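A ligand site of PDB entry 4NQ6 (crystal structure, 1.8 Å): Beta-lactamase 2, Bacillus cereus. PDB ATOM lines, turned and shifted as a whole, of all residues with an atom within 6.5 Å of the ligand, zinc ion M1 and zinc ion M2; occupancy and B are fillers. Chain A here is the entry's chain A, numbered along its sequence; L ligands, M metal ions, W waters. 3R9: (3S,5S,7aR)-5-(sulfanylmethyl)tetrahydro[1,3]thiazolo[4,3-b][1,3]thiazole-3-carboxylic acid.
The side-chain amino group (NZ) of Lys 166 is in salt-bridge range of an oxygen (O) of the ligand, at 2.9 Å.
A sulfur (SAC) of the ligand sits close to the side-chain carboxylate of Asp 85.
A ring nitrogen (ND1) of His 205 is in hydrogen-bond range of the backbone carbonyl oxygen (O) of Pro 35.
SG of Cys 163 lies close to NH1 of Arg 86 (3.4 Å).
The backbone carbonyl oxygen of Leu 173 is in hydrogen-bond range of the side-chain amino group of Lys 166, 3.0 Å away.
The side-chain carboxylate (OD2) of Asp 85 lies within salt-bridge range of the guanidinium group (NE) of Arg 86 (3.3 Å).
OG of Ser 36 is in hydrogen-bond range of OD1 of Asp 85, at 2.7 Å.
Residues that only touch the ligand: Phe 29, Val 34, Trp 54, Leu 173, Gly 174 and Asn 175.
Hydrophobic or aromatic side chains that line the ligand: Phe 29, Val 34, Trp 54, His 83, His 144 and His 205.
13 residues have an atom within 4 Å of the ligand: Phe 29, Val 34, Trp 54, His 81, His 83, Asp 85, His 144, Cys 163, Lys 166, Leu 173, Gly 174, Asn 175 and His 205.
Of the 23 residues printed, 3 come within 4 Å of zinc ion M1.
Merely in contact with zinc ion M2: Asp 85 (3.9 Å).
Of the 23 residues printed, 3 come within 4 Å of zinc ion M2.
The nearest printed residue that does not touch zinc ion M2 is His 144 (4.2 Å).
Zinc ion M1 is bound by a ring nitrogen (ND1) of His 83 (2.1 Å), a ring nitrogen (NE2) of His 144 (2.1 Å), a ring nitrogen (NE2) of His 81 (2.1 Å) and a sulfur (SAC) of the ligand (2.3 Å).
Zinc ion M1 has four donor atoms within binding distance.
OXT of the ligand is bound to zinc ion M2, 2.0 Å away.
NE2 of His 205 binds zinc ion M2, at 2.1 Å.
SAC of the ligand is bound to zinc ion M2, 2.3 Å away.
SG of Cys 163 is bound to zinc ion M2 (2.3 Å).
Zinc ion M2 has four donor atoms within binding distance.
Slightly farther from zinc ion M2 lies a nitrogen (N) of the ligand (2.7 Å).
Water W1 lies within hydrogen-bond range of the backbone carbonyl oxygen (O) of Cys 163, the side-chain amino group (NZ) of Lys 166 and an oxygen (O) of the ligand.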
ATOM      1  N   PHE A  29       9.572 -25.618  14.469  1.00  0.00           N
ATOM      2  CA  PHE A  29       9.733 -25.449  13.019  1.00  0.00           C
ATOM      3  C   PHE A  29       8.345 -25.501  12.313  1.00  0.00           C
ATOM      4  O   PHE A  29       7.400 -24.906  12.831  1.00  0.00           O
ATOM      5  CB  PHE A  29      10.773 -26.465  12.469  1.00  0.00           C
ATOM      6  CG  PHE A  29      11.433 -26.017  11.171  1.00  0.00           C
ATOM      7  CD1 PHE A  29      12.160 -24.826  11.121  1.00  0.00           C
ATOM      8  CD2 PHE A  29      11.352 -26.804  10.013  1.00  0.00           C
ATOM      9  CE1 PHE A  29      12.757 -24.414   9.938  1.00  0.00           C
ATOM     10  CE2 PHE A  29      11.938 -26.390   8.821  1.00  0.00           C
ATOM     11  CZ  PHE A  29      12.647 -25.191   8.782  1.00  0.00           C
ATOM     12  N   VAL A  34      10.663 -29.827  16.894  1.00  0.00           N
ATOM     13  CA  VAL A  34      11.786 -30.420  16.129  1.00  0.00           C
ATOM     14  C   VAL A  34      13.097 -30.367  16.906  1.00  0.00           C
ATOM     15  O   VAL A  34      13.538 -29.273  17.282  1.00  0.00           O
ATOM     16  CB  VAL A  34      12.040 -29.676  14.807  1.00  0.00           C
ATOM     17  CG1 VAL A  34      12.907 -30.533  13.879  1.00  0.00           C
ATOM     18  CG2 VAL A  34      10.732 -29.252  14.174  1.00  0.00           C
ATOM     19  N   PRO A  35      13.741 -31.524  17.127  1.00  0.00           N
ATOM     20  CA  PRO A  35      14.913 -31.430  17.977  1.00  0.00           C
ATOM     21  C   PRO A  35      16.183 -31.083  17.219  1.00  0.00           C
ATOM     22  O   PRO A  35      16.348 -31.485  16.056  1.00  0.00           O
ATOM     23  CB  PRO A  35      15.028 -32.827  18.574  1.00  0.00           C
ATOM     24  CG  PRO A  35      14.437 -33.713  17.545  1.00  0.00           C
ATOM     25  CD  PRO A  35      13.352 -32.913  16.890  1.00  0.00           C
ATOM     26  N   SER A  36      17.078 -30.391  17.923  1.00  0.00           N
ATOM     27  CA  SER A  36      18.355 -29.942  17.394  1.00  0.00           C
ATOM     28  C   SER A  36      19.443 -30.358  18.379  1.00  0.00           C
ATOM     29  O   SER A  36      19.304 -30.093  19.580  1.00  0.00           O
ATOM     30  CB  SER A  36      18.296 -28.406  17.248  1.00  0.00           C
ATOM     31  OG  SER A  36      19.504 -27.873  16.726  1.00  0.00           O
ATOM     32  N   TRP A  54      18.212 -22.862  18.973  1.00  0.00           N
ATOM     33  CA  TRP A  54      17.262 -22.234  18.032  1.00  0.00           C
ATOM     34  C   TRP A  54      17.125 -20.722  18.154  1.00  0.00           C
ATOM     35  O   TRP A  54      16.995 -20.023  17.161  1.00  0.00           O
ATOM     36  CB  TRP A  54      15.820 -22.835  18.227  1.00  0.00           C
ATOM     37  CG  TRP A  54      15.679 -24.270  17.874  1.00  0.00           C
ATOM     38  CD1 TRP A  54      15.857 -25.336  18.710  1.00  0.00           C
ATOM     39  CD2 TRP A  54      15.320 -24.825  16.584  1.00  0.00           C
ATOM     40  NE1 TRP A  54      15.647 -26.518  18.023  1.00  0.00           N
ATOM     41  CE2 TRP A  54      15.328 -26.244  16.719  1.00  0.00           C
ATOM     42  CE3 TRP A  54      15.003 -24.269  15.330  1.00  0.00           C
ATOM     43  CZ2 TRP A  54      15.031 -27.113  15.651  1.00  0.00           C
ATOM     44  CZ3 TRP A  54      14.684 -25.142  14.265  1.00  0.00           C
ATOM     45  CH2 TRP A  54      14.713 -26.538  14.446  1.00  0.00           C
ATOM     46  N   HIS A  81      26.949 -23.707  11.173  1.00  0.00           N
ATOM     47  CA  HIS A  81      26.568 -22.954   9.980  1.00  0.00           C
ATOM     48  C   HIS A  81      25.571 -21.846  10.349  1.00  0.00           C
ATOM     49  O   HIS A  81      25.242 -21.651  11.512  1.00  0.00           O
ATOM     50  CB  HIS A  81      26.025 -23.855   8.825  1.00  0.00           C
ATOM     51  CG  HIS A  81      24.773 -24.598   9.160  1.00  0.00           C
ATOM     52  ND1 HIS A  81      24.767 -25.734   9.917  1.00  0.00           N
ATOM     53  CD2 HIS A  81      23.481 -24.408   8.773  1.00  0.00           C
ATOM     54  CE1 HIS A  81      23.540 -26.213  10.007  1.00  0.00           C
ATOM     55  NE2 HIS A  81      22.740 -25.424   9.308  1.00  0.00           N
ATOM     56  N   ALA A  82      25.075 -21.112   9.346  1.00  0.00           N
ATOM     57  CA  ALA A  82      24.383 -19.849   9.573  1.00  0.00           C
ATOM     58  C   ALA A  82      22.865 -19.951   9.501  1.00  0.00           C
ATOM     59  O   ALA A  82      22.180 -18.950   9.459  1.00  0.00           O
ATOM     60  CB  ALA A  82      24.864 -18.812   8.588  1.00  0.00           C
ATOM     61  N   HIS A  83      22.309 -21.122   9.517  1.00  0.00           N
ATOM     62  CA  HIS A  83      20.882 -21.234   9.699  1.00  0.00           C
ATOM     63  C   HIS A  83      20.508 -20.833  11.123  1.00  0.00           C
ATOM     64  O   HIS A  83      21.259 -21.107  12.088  1.00  0.00           O
ATOM     65  CB  HIS A  83      20.379 -22.648   9.439  1.00  0.00           C
ATOM     66  CG  HIS A  83      20.165 -22.945   7.992  1.00  0.00           C
ATOM     67  ND1 HIS A  83      20.266 -24.215   7.462  1.00  0.00           N
ATOM     68  CD2 HIS A  83      19.990 -22.096   6.942  1.00  0.00           C
ATOM     69  CE1 HIS A  83      20.032 -24.152   6.169  1.00  0.00           C
ATOM     70  NE2 HIS A  83      19.870 -22.885   5.830  1.00  0.00           N
ATOM     71  N   ALA A  84      19.284 -20.298  11.237  1.00  0.00           N
ATOM     72  CA  ALA A  84      18.697 -19.900  12.493  1.00  0.00           C
ATOM     73  C   ALA A  84      18.854 -20.967  13.587  1.00  0.00           C
ATOM     74  O   ALA A  84      19.135 -20.652  14.769  1.00  0.00           O
ATOM     75  CB  ALA A  84      17.206 -19.548  12.290  1.00  0.00           C
ATOM     76  N   ASP A  85      18.697 -22.233  13.211  1.00  0.00           N
ATOM     77  CA  ASP A  85      18.866 -23.334  14.196  1.00  0.00           C
ATOM     78  C   ASP A  85      20.209 -23.318  14.985  1.00  0.00           C
ATOM     79  O   ASP A  85      20.269 -23.686  16.131  1.00  0.00           O
ATOM     80  CB  ASP A  85      18.750 -24.686  13.462  1.00  0.00           C
ATOM     81  CG  ASP A  85      18.862 -25.857  14.382  1.00  0.00           C
ATOM     82  OD1 ASP A  85      18.262 -25.809  15.427  1.00  0.00           O
ATOM     83  OD2 ASP A  85      19.539 -26.857  14.068  1.00  0.00           O
ATOM     84  N   ARG A  86      21.275 -22.936  14.288  1.00  0.00           N
ATOM     85  CA  ARG A  86      22.656 -22.834  14.856  1.00  0.00           C
ATOM     86  C   ARG A  86      23.054 -21.414  15.342  1.00  0.00           C
ATOM     87  O   ARG A  86      23.737 -21.284  16.338  1.00  0.00           O
ATOM     88  CB  ARG A  86      23.654 -23.263  13.756  1.00  0.00           C
ATOM     89  CG  ARG A  86      23.358 -24.613  13.115  1.00  0.00           C
ATOM     90  CD  ARG A  86      23.075 -25.612  14.212  1.00  0.00           C
ATOM     91  NE  ARG A  86      22.858 -26.984  13.859  1.00  0.00           N
ATOM     92  CZ  ARG A  86      22.555 -27.927  14.768  1.00  0.00           C
ATOM     93  NH1 ARG A  86      22.323 -29.170  14.408  1.00  0.00           N
ATOM     94  NH2 ARG A  86      22.500 -27.649  16.047  1.00  0.00           N
ATOM     95  N   HIS A 144      24.717 -29.661   3.116  1.00  0.00           N
ATOM     96  CA  HIS A 144      23.462 -29.175   3.668  1.00  0.00           C
ATOM     97  C   HIS A 144      23.319 -27.631   3.491  1.00  0.00           C
ATOM     98  O   HIS A 144      22.265 -27.145   3.184  1.00  0.00           O
ATOM     99  CB  HIS A 144      23.372 -29.538   5.138  1.00  0.00           C
ATOM    100  CG  HIS A 144      22.349 -28.734   5.880  1.00  0.00           C
ATOM    101  ND1 HIS A 144      21.001 -28.956   5.753  1.00  0.00           N
ATOM    102  CD2 HIS A 144      22.488 -27.702   6.740  1.00  0.00           C
ATOM    103  CE1 HIS A 144      20.352 -28.139   6.549  1.00  0.00           C
ATOM    104  NE2 HIS A 144      21.222 -27.356   7.141  1.00  0.00           N
ATOM    105  N   THR A 145      24.431 -26.905   3.665  1.00  0.00           N
ATOM    106  CA  THR A 145      24.561 -25.515   3.282  1.00  0.00           C
ATOM    107  C   THR A 145      25.949 -25.318   2.695  1.00  0.00           C
ATOM    108  O   THR A 145      26.789 -26.208   2.711  1.00  0.00           O
ATOM    109  CB  THR A 145      24.430 -24.537   4.479  1.00  0.00           C
ATOM    110  OG1 THR A 145      25.360 -24.926   5.490  1.00  0.00           O
ATOM    111  CG2 THR A 145      23.026 -24.448   4.996  1.00  0.00           C
ATOM    112  N   GLY A 162      26.811 -32.182  12.643  1.00  0.00           N
ATOM    113  CA  GLY A 162      25.913 -31.078  12.318  1.00  0.00           C
ATOM    114  C   GLY A 162      24.914 -31.485  11.229  1.00  0.00           C
ATOM    115  O   GLY A 162      24.666 -32.704  10.979  1.00  0.00           O
ATOM    116  N   CYS A 163      24.350 -30.496  10.543  1.00  0.00           N
ATOM    117  CA  CYS A 163      23.278 -30.801   9.610  1.00  0.00           C
ATOM    118  C   CYS A 163      23.731 -31.459   8.286  1.00  0.00           C
ATOM    119  O   CYS A 163      22.933 -31.953   7.541  1.00  0.00           O
ATOM    120  CB  CYS A 163      22.291 -29.628   9.480  1.00  0.00           C
ATOM    121  SG  CYS A 163      21.739 -29.035  11.111  1.00  0.00           S
ATOM    122  N   LEU A 164      25.048 -31.495   8.047  1.00  0.00           N
ATOM    123  CA  LEU A 164      25.650 -32.260   6.995  1.00  0.00           C
ATOM    124  C   LEU A 164      25.307 -33.733   7.120  1.00  0.00           C
ATOM    125  O   LEU A 164      25.340 -34.458   6.122  1.00  0.00           O
ATOM    126  CB  LEU A 164      27.166 -32.074   7.004  1.00  0.00           C
ATOM    127  CG  LEU A 164      27.973 -32.641   5.847  1.00  0.00           C
ATOM    128  CD1 LEU A 164      27.822 -31.856   4.539  1.00  0.00           C
ATOM    129  CD2 LEU A 164      29.406 -32.776   6.229  1.00  0.00           C
ATOM    130  N   LYS A 166      22.849 -36.790   8.431  1.00  0.00           N
ATOM    131  CA  LYS A 166      21.468 -37.189   8.783  1.00  0.00           C
ATOM    132  C   LYS A 166      21.414 -38.369   9.746  1.00  0.00           C
ATOM    133  O   LYS A 166      22.236 -39.235   9.700  1.00  0.00           O
ATOM    134  CB  LYS A 166      20.677 -37.541   7.496  1.00  0.00           C
ATOM    135  CG  LYS A 166      20.698 -36.445   6.427  1.00  0.00           C
ATOM    136  CD  LYS A 166      20.328 -35.097   6.979  1.00  0.00           C
ATOM    137  CE  LYS A 166      18.846 -34.910   7.216  1.00  0.00           C
ATOM    138  NZ  LYS A 166      18.476 -33.443   7.088  1.00  0.00           N
ATOM    139  N   LEU A 173      16.469 -35.722   2.711  1.00  0.00           N
ATOM    140  CA  LEU A 173      17.482 -34.730   3.042  1.00  0.00           C
ATOM    141  C   LEU A 173      17.015 -33.501   3.836  1.00  0.00           C
ATOM    142  O   LEU A 173      17.869 -32.730   4.279  1.00  0.00           O
ATOM    143  CB  LEU A 173      18.228 -34.294   1.806  1.00  0.00           C
ATOM    144  CG  LEU A 173      19.002 -35.432   1.113  1.00  0.00           C
ATOM    145  CD1 LEU A 173      19.326 -34.995  -0.294  1.00  0.00           C
ATOM    146  CD2 LEU A 173      20.213 -35.840   1.919  1.00  0.00           C
ATOM    147  N   GLY A 174      15.701 -33.348   4.088  1.00  0.00           N
ATOM    148  CA  GLY A 174      15.234 -32.192   4.883  1.00  0.00           C
ATOM    149  C   GLY A 174      15.074 -31.000   3.955  1.00  0.00           C
ATOM    150  O   GLY A 174      14.793 -31.169   2.762  1.00  0.00           O
ATOM    151  N   ASN A 175      15.264 -29.795   4.448  1.00  0.00           N
ATOM    152  CA  ASN A 175      15.123 -28.656   3.545  1.00  0.00           C
ATOM    153  C   ASN A 175      16.412 -28.490   2.751  1.00  0.00           C
ATOM    154  O   ASN A 175      17.473 -28.340   3.330  1.00  0.00           O
ATOM    155  CB  ASN A 175      14.797 -27.352   4.271  1.00  0.00           C
ATOM    156  CG  ASN A 175      14.610 -26.178   3.318  1.00  0.00           C
ATOM    157  OD1 ASN A 175      13.516 -25.950   2.799  1.00  0.00           O
ATOM    158  ND2 ASN A 175      15.672 -25.437   3.088  1.00  0.00           N
ATOM    159  N   TRP A 184      27.465 -32.346  -1.821  1.00  0.00           N
ATOM    160  CA  TRP A 184      27.256 -32.935  -0.497  1.00  0.00           C
ATOM    161  C   TRP A 184      27.919 -34.319  -0.397  1.00  0.00           C
ATOM    162  O   TRP A 184      28.523 -34.688   0.641  1.00  0.00           O
ATOM    163  CB  TRP A 184      25.755 -33.001  -0.231  1.00  0.00           C
ATOM    164  CG  TRP A 184      25.297 -33.139   1.170  1.00  0.00           C
ATOM    165  CD1 TRP A 184      25.982 -33.705   2.227  1.00  0.00           C
ATOM    166  CD2 TRP A 184      23.994 -32.805   1.679  1.00  0.00           C
ATOM    167  NE1 TRP A 184      25.191 -33.719   3.335  1.00  0.00           N
ATOM    168  CE2 TRP A 184      23.970 -33.164   3.038  1.00  0.00           C
ATOM    169  CE3 TRP A 184      22.834 -32.252   1.111  1.00  0.00           C
ATOM    170  CZ2 TRP A 184      22.833 -33.024   3.840  1.00  0.00           C
ATOM    171  CZ3 TRP A 184      21.728 -32.078   1.915  1.00  0.00           C
ATOM    172  CH2 TRP A 184      21.732 -32.445   3.271  1.00  0.00           C
ATOM    173  N   GLY A 204      23.032 -33.483  13.159  1.00  0.00           N
ATOM    174  CA  GLY A 204      22.457 -32.170  13.496  1.00  0.00           C
ATOM    175  C   GLY A 204      21.137 -32.338  14.295  1.00  0.00           C
ATOM    176  O   GLY A 204      20.829 -31.558  15.176  1.00  0.00           O
ATOM    177  N   HIS A 205      20.358 -33.326  13.874  1.00  0.00           N
ATOM    178  CA  HIS A 205      19.089 -33.686  14.440  1.00  0.00           C
ATOM    179  C   HIS A 205      19.039 -35.230  14.560  1.00  0.00           C
ATOM    180  O   HIS A 205      19.377 -35.957  13.606  1.00  0.00           O
ATOM    181  CB  HIS A 205      17.970 -33.211  13.501  1.00  0.00           C
ATOM    182  CG  HIS A 205      18.077 -31.753  13.112  1.00  0.00           C
ATOM    183  ND1 HIS A 205      17.690 -30.728  13.946  1.00  0.00           N
ATOM    184  CD2 HIS A 205      18.588 -31.156  12.004  1.00  0.00           C
ATOM    185  CE1 HIS A 205      17.916 -29.568  13.372  1.00  0.00           C
ATOM    186  NE2 HIS A 205      18.454 -29.792  12.188  1.00  0.00           N
HETATM  187  O   3R9 L   1      17.630 -30.673   7.501  1.00  0.00           O
HETATM  188  N   3R9 L   1      17.034 -27.927   9.800  1.00  0.00           N
HETATM  189  C   3R9 L   1      17.829 -29.933   8.468  1.00  0.00           C
HETATM  190  OXT 3R9 L   1      18.930 -29.838   9.091  1.00  0.00           O
HETATM  191  CA  3R9 L   1      16.587 -29.034   8.877  1.00  0.00           C
HETATM  192  CB  3R9 L   1      15.400 -29.842   9.478  1.00  0.00           C
HETATM  193  SAH 3R9 L   1      15.178 -29.199  11.132  1.00  0.00           S
HETATM  194  CAM 3R9 L   1      16.180 -27.725  11.027  1.00  0.00           C
HETATM  195  CAF 3R9 L   1      15.238 -26.561  10.851  1.00  0.00           C
HETATM  196  SAG 3R9 L   1      15.327 -26.435   9.060  1.00  0.00           S
HETATM  197  CAJ 3R9 L   1      17.073 -26.696   8.984  1.00  0.00           C
HETATM  198  CAD 3R9 L   1      17.877 -25.619   9.643  1.00  0.00           C
HETATM  199  SAC 3R9 L   1      19.378 -26.427  10.309  1.00  0.00           S
HETATM  200 ZN    ZN M   1      20.834 -25.886   8.573  1.00  0.00          ZN
HETATM  201 ZN    ZN M   2      19.453 -28.728  10.677  1.00  0.00          ZN
HETATM  202  O   HOH W   1      20.395 -32.199   8.797  1.00  0.00           O
HETATM  203  O   HOH W   2      16.925 -22.948  11.041  1.00  0.00           O
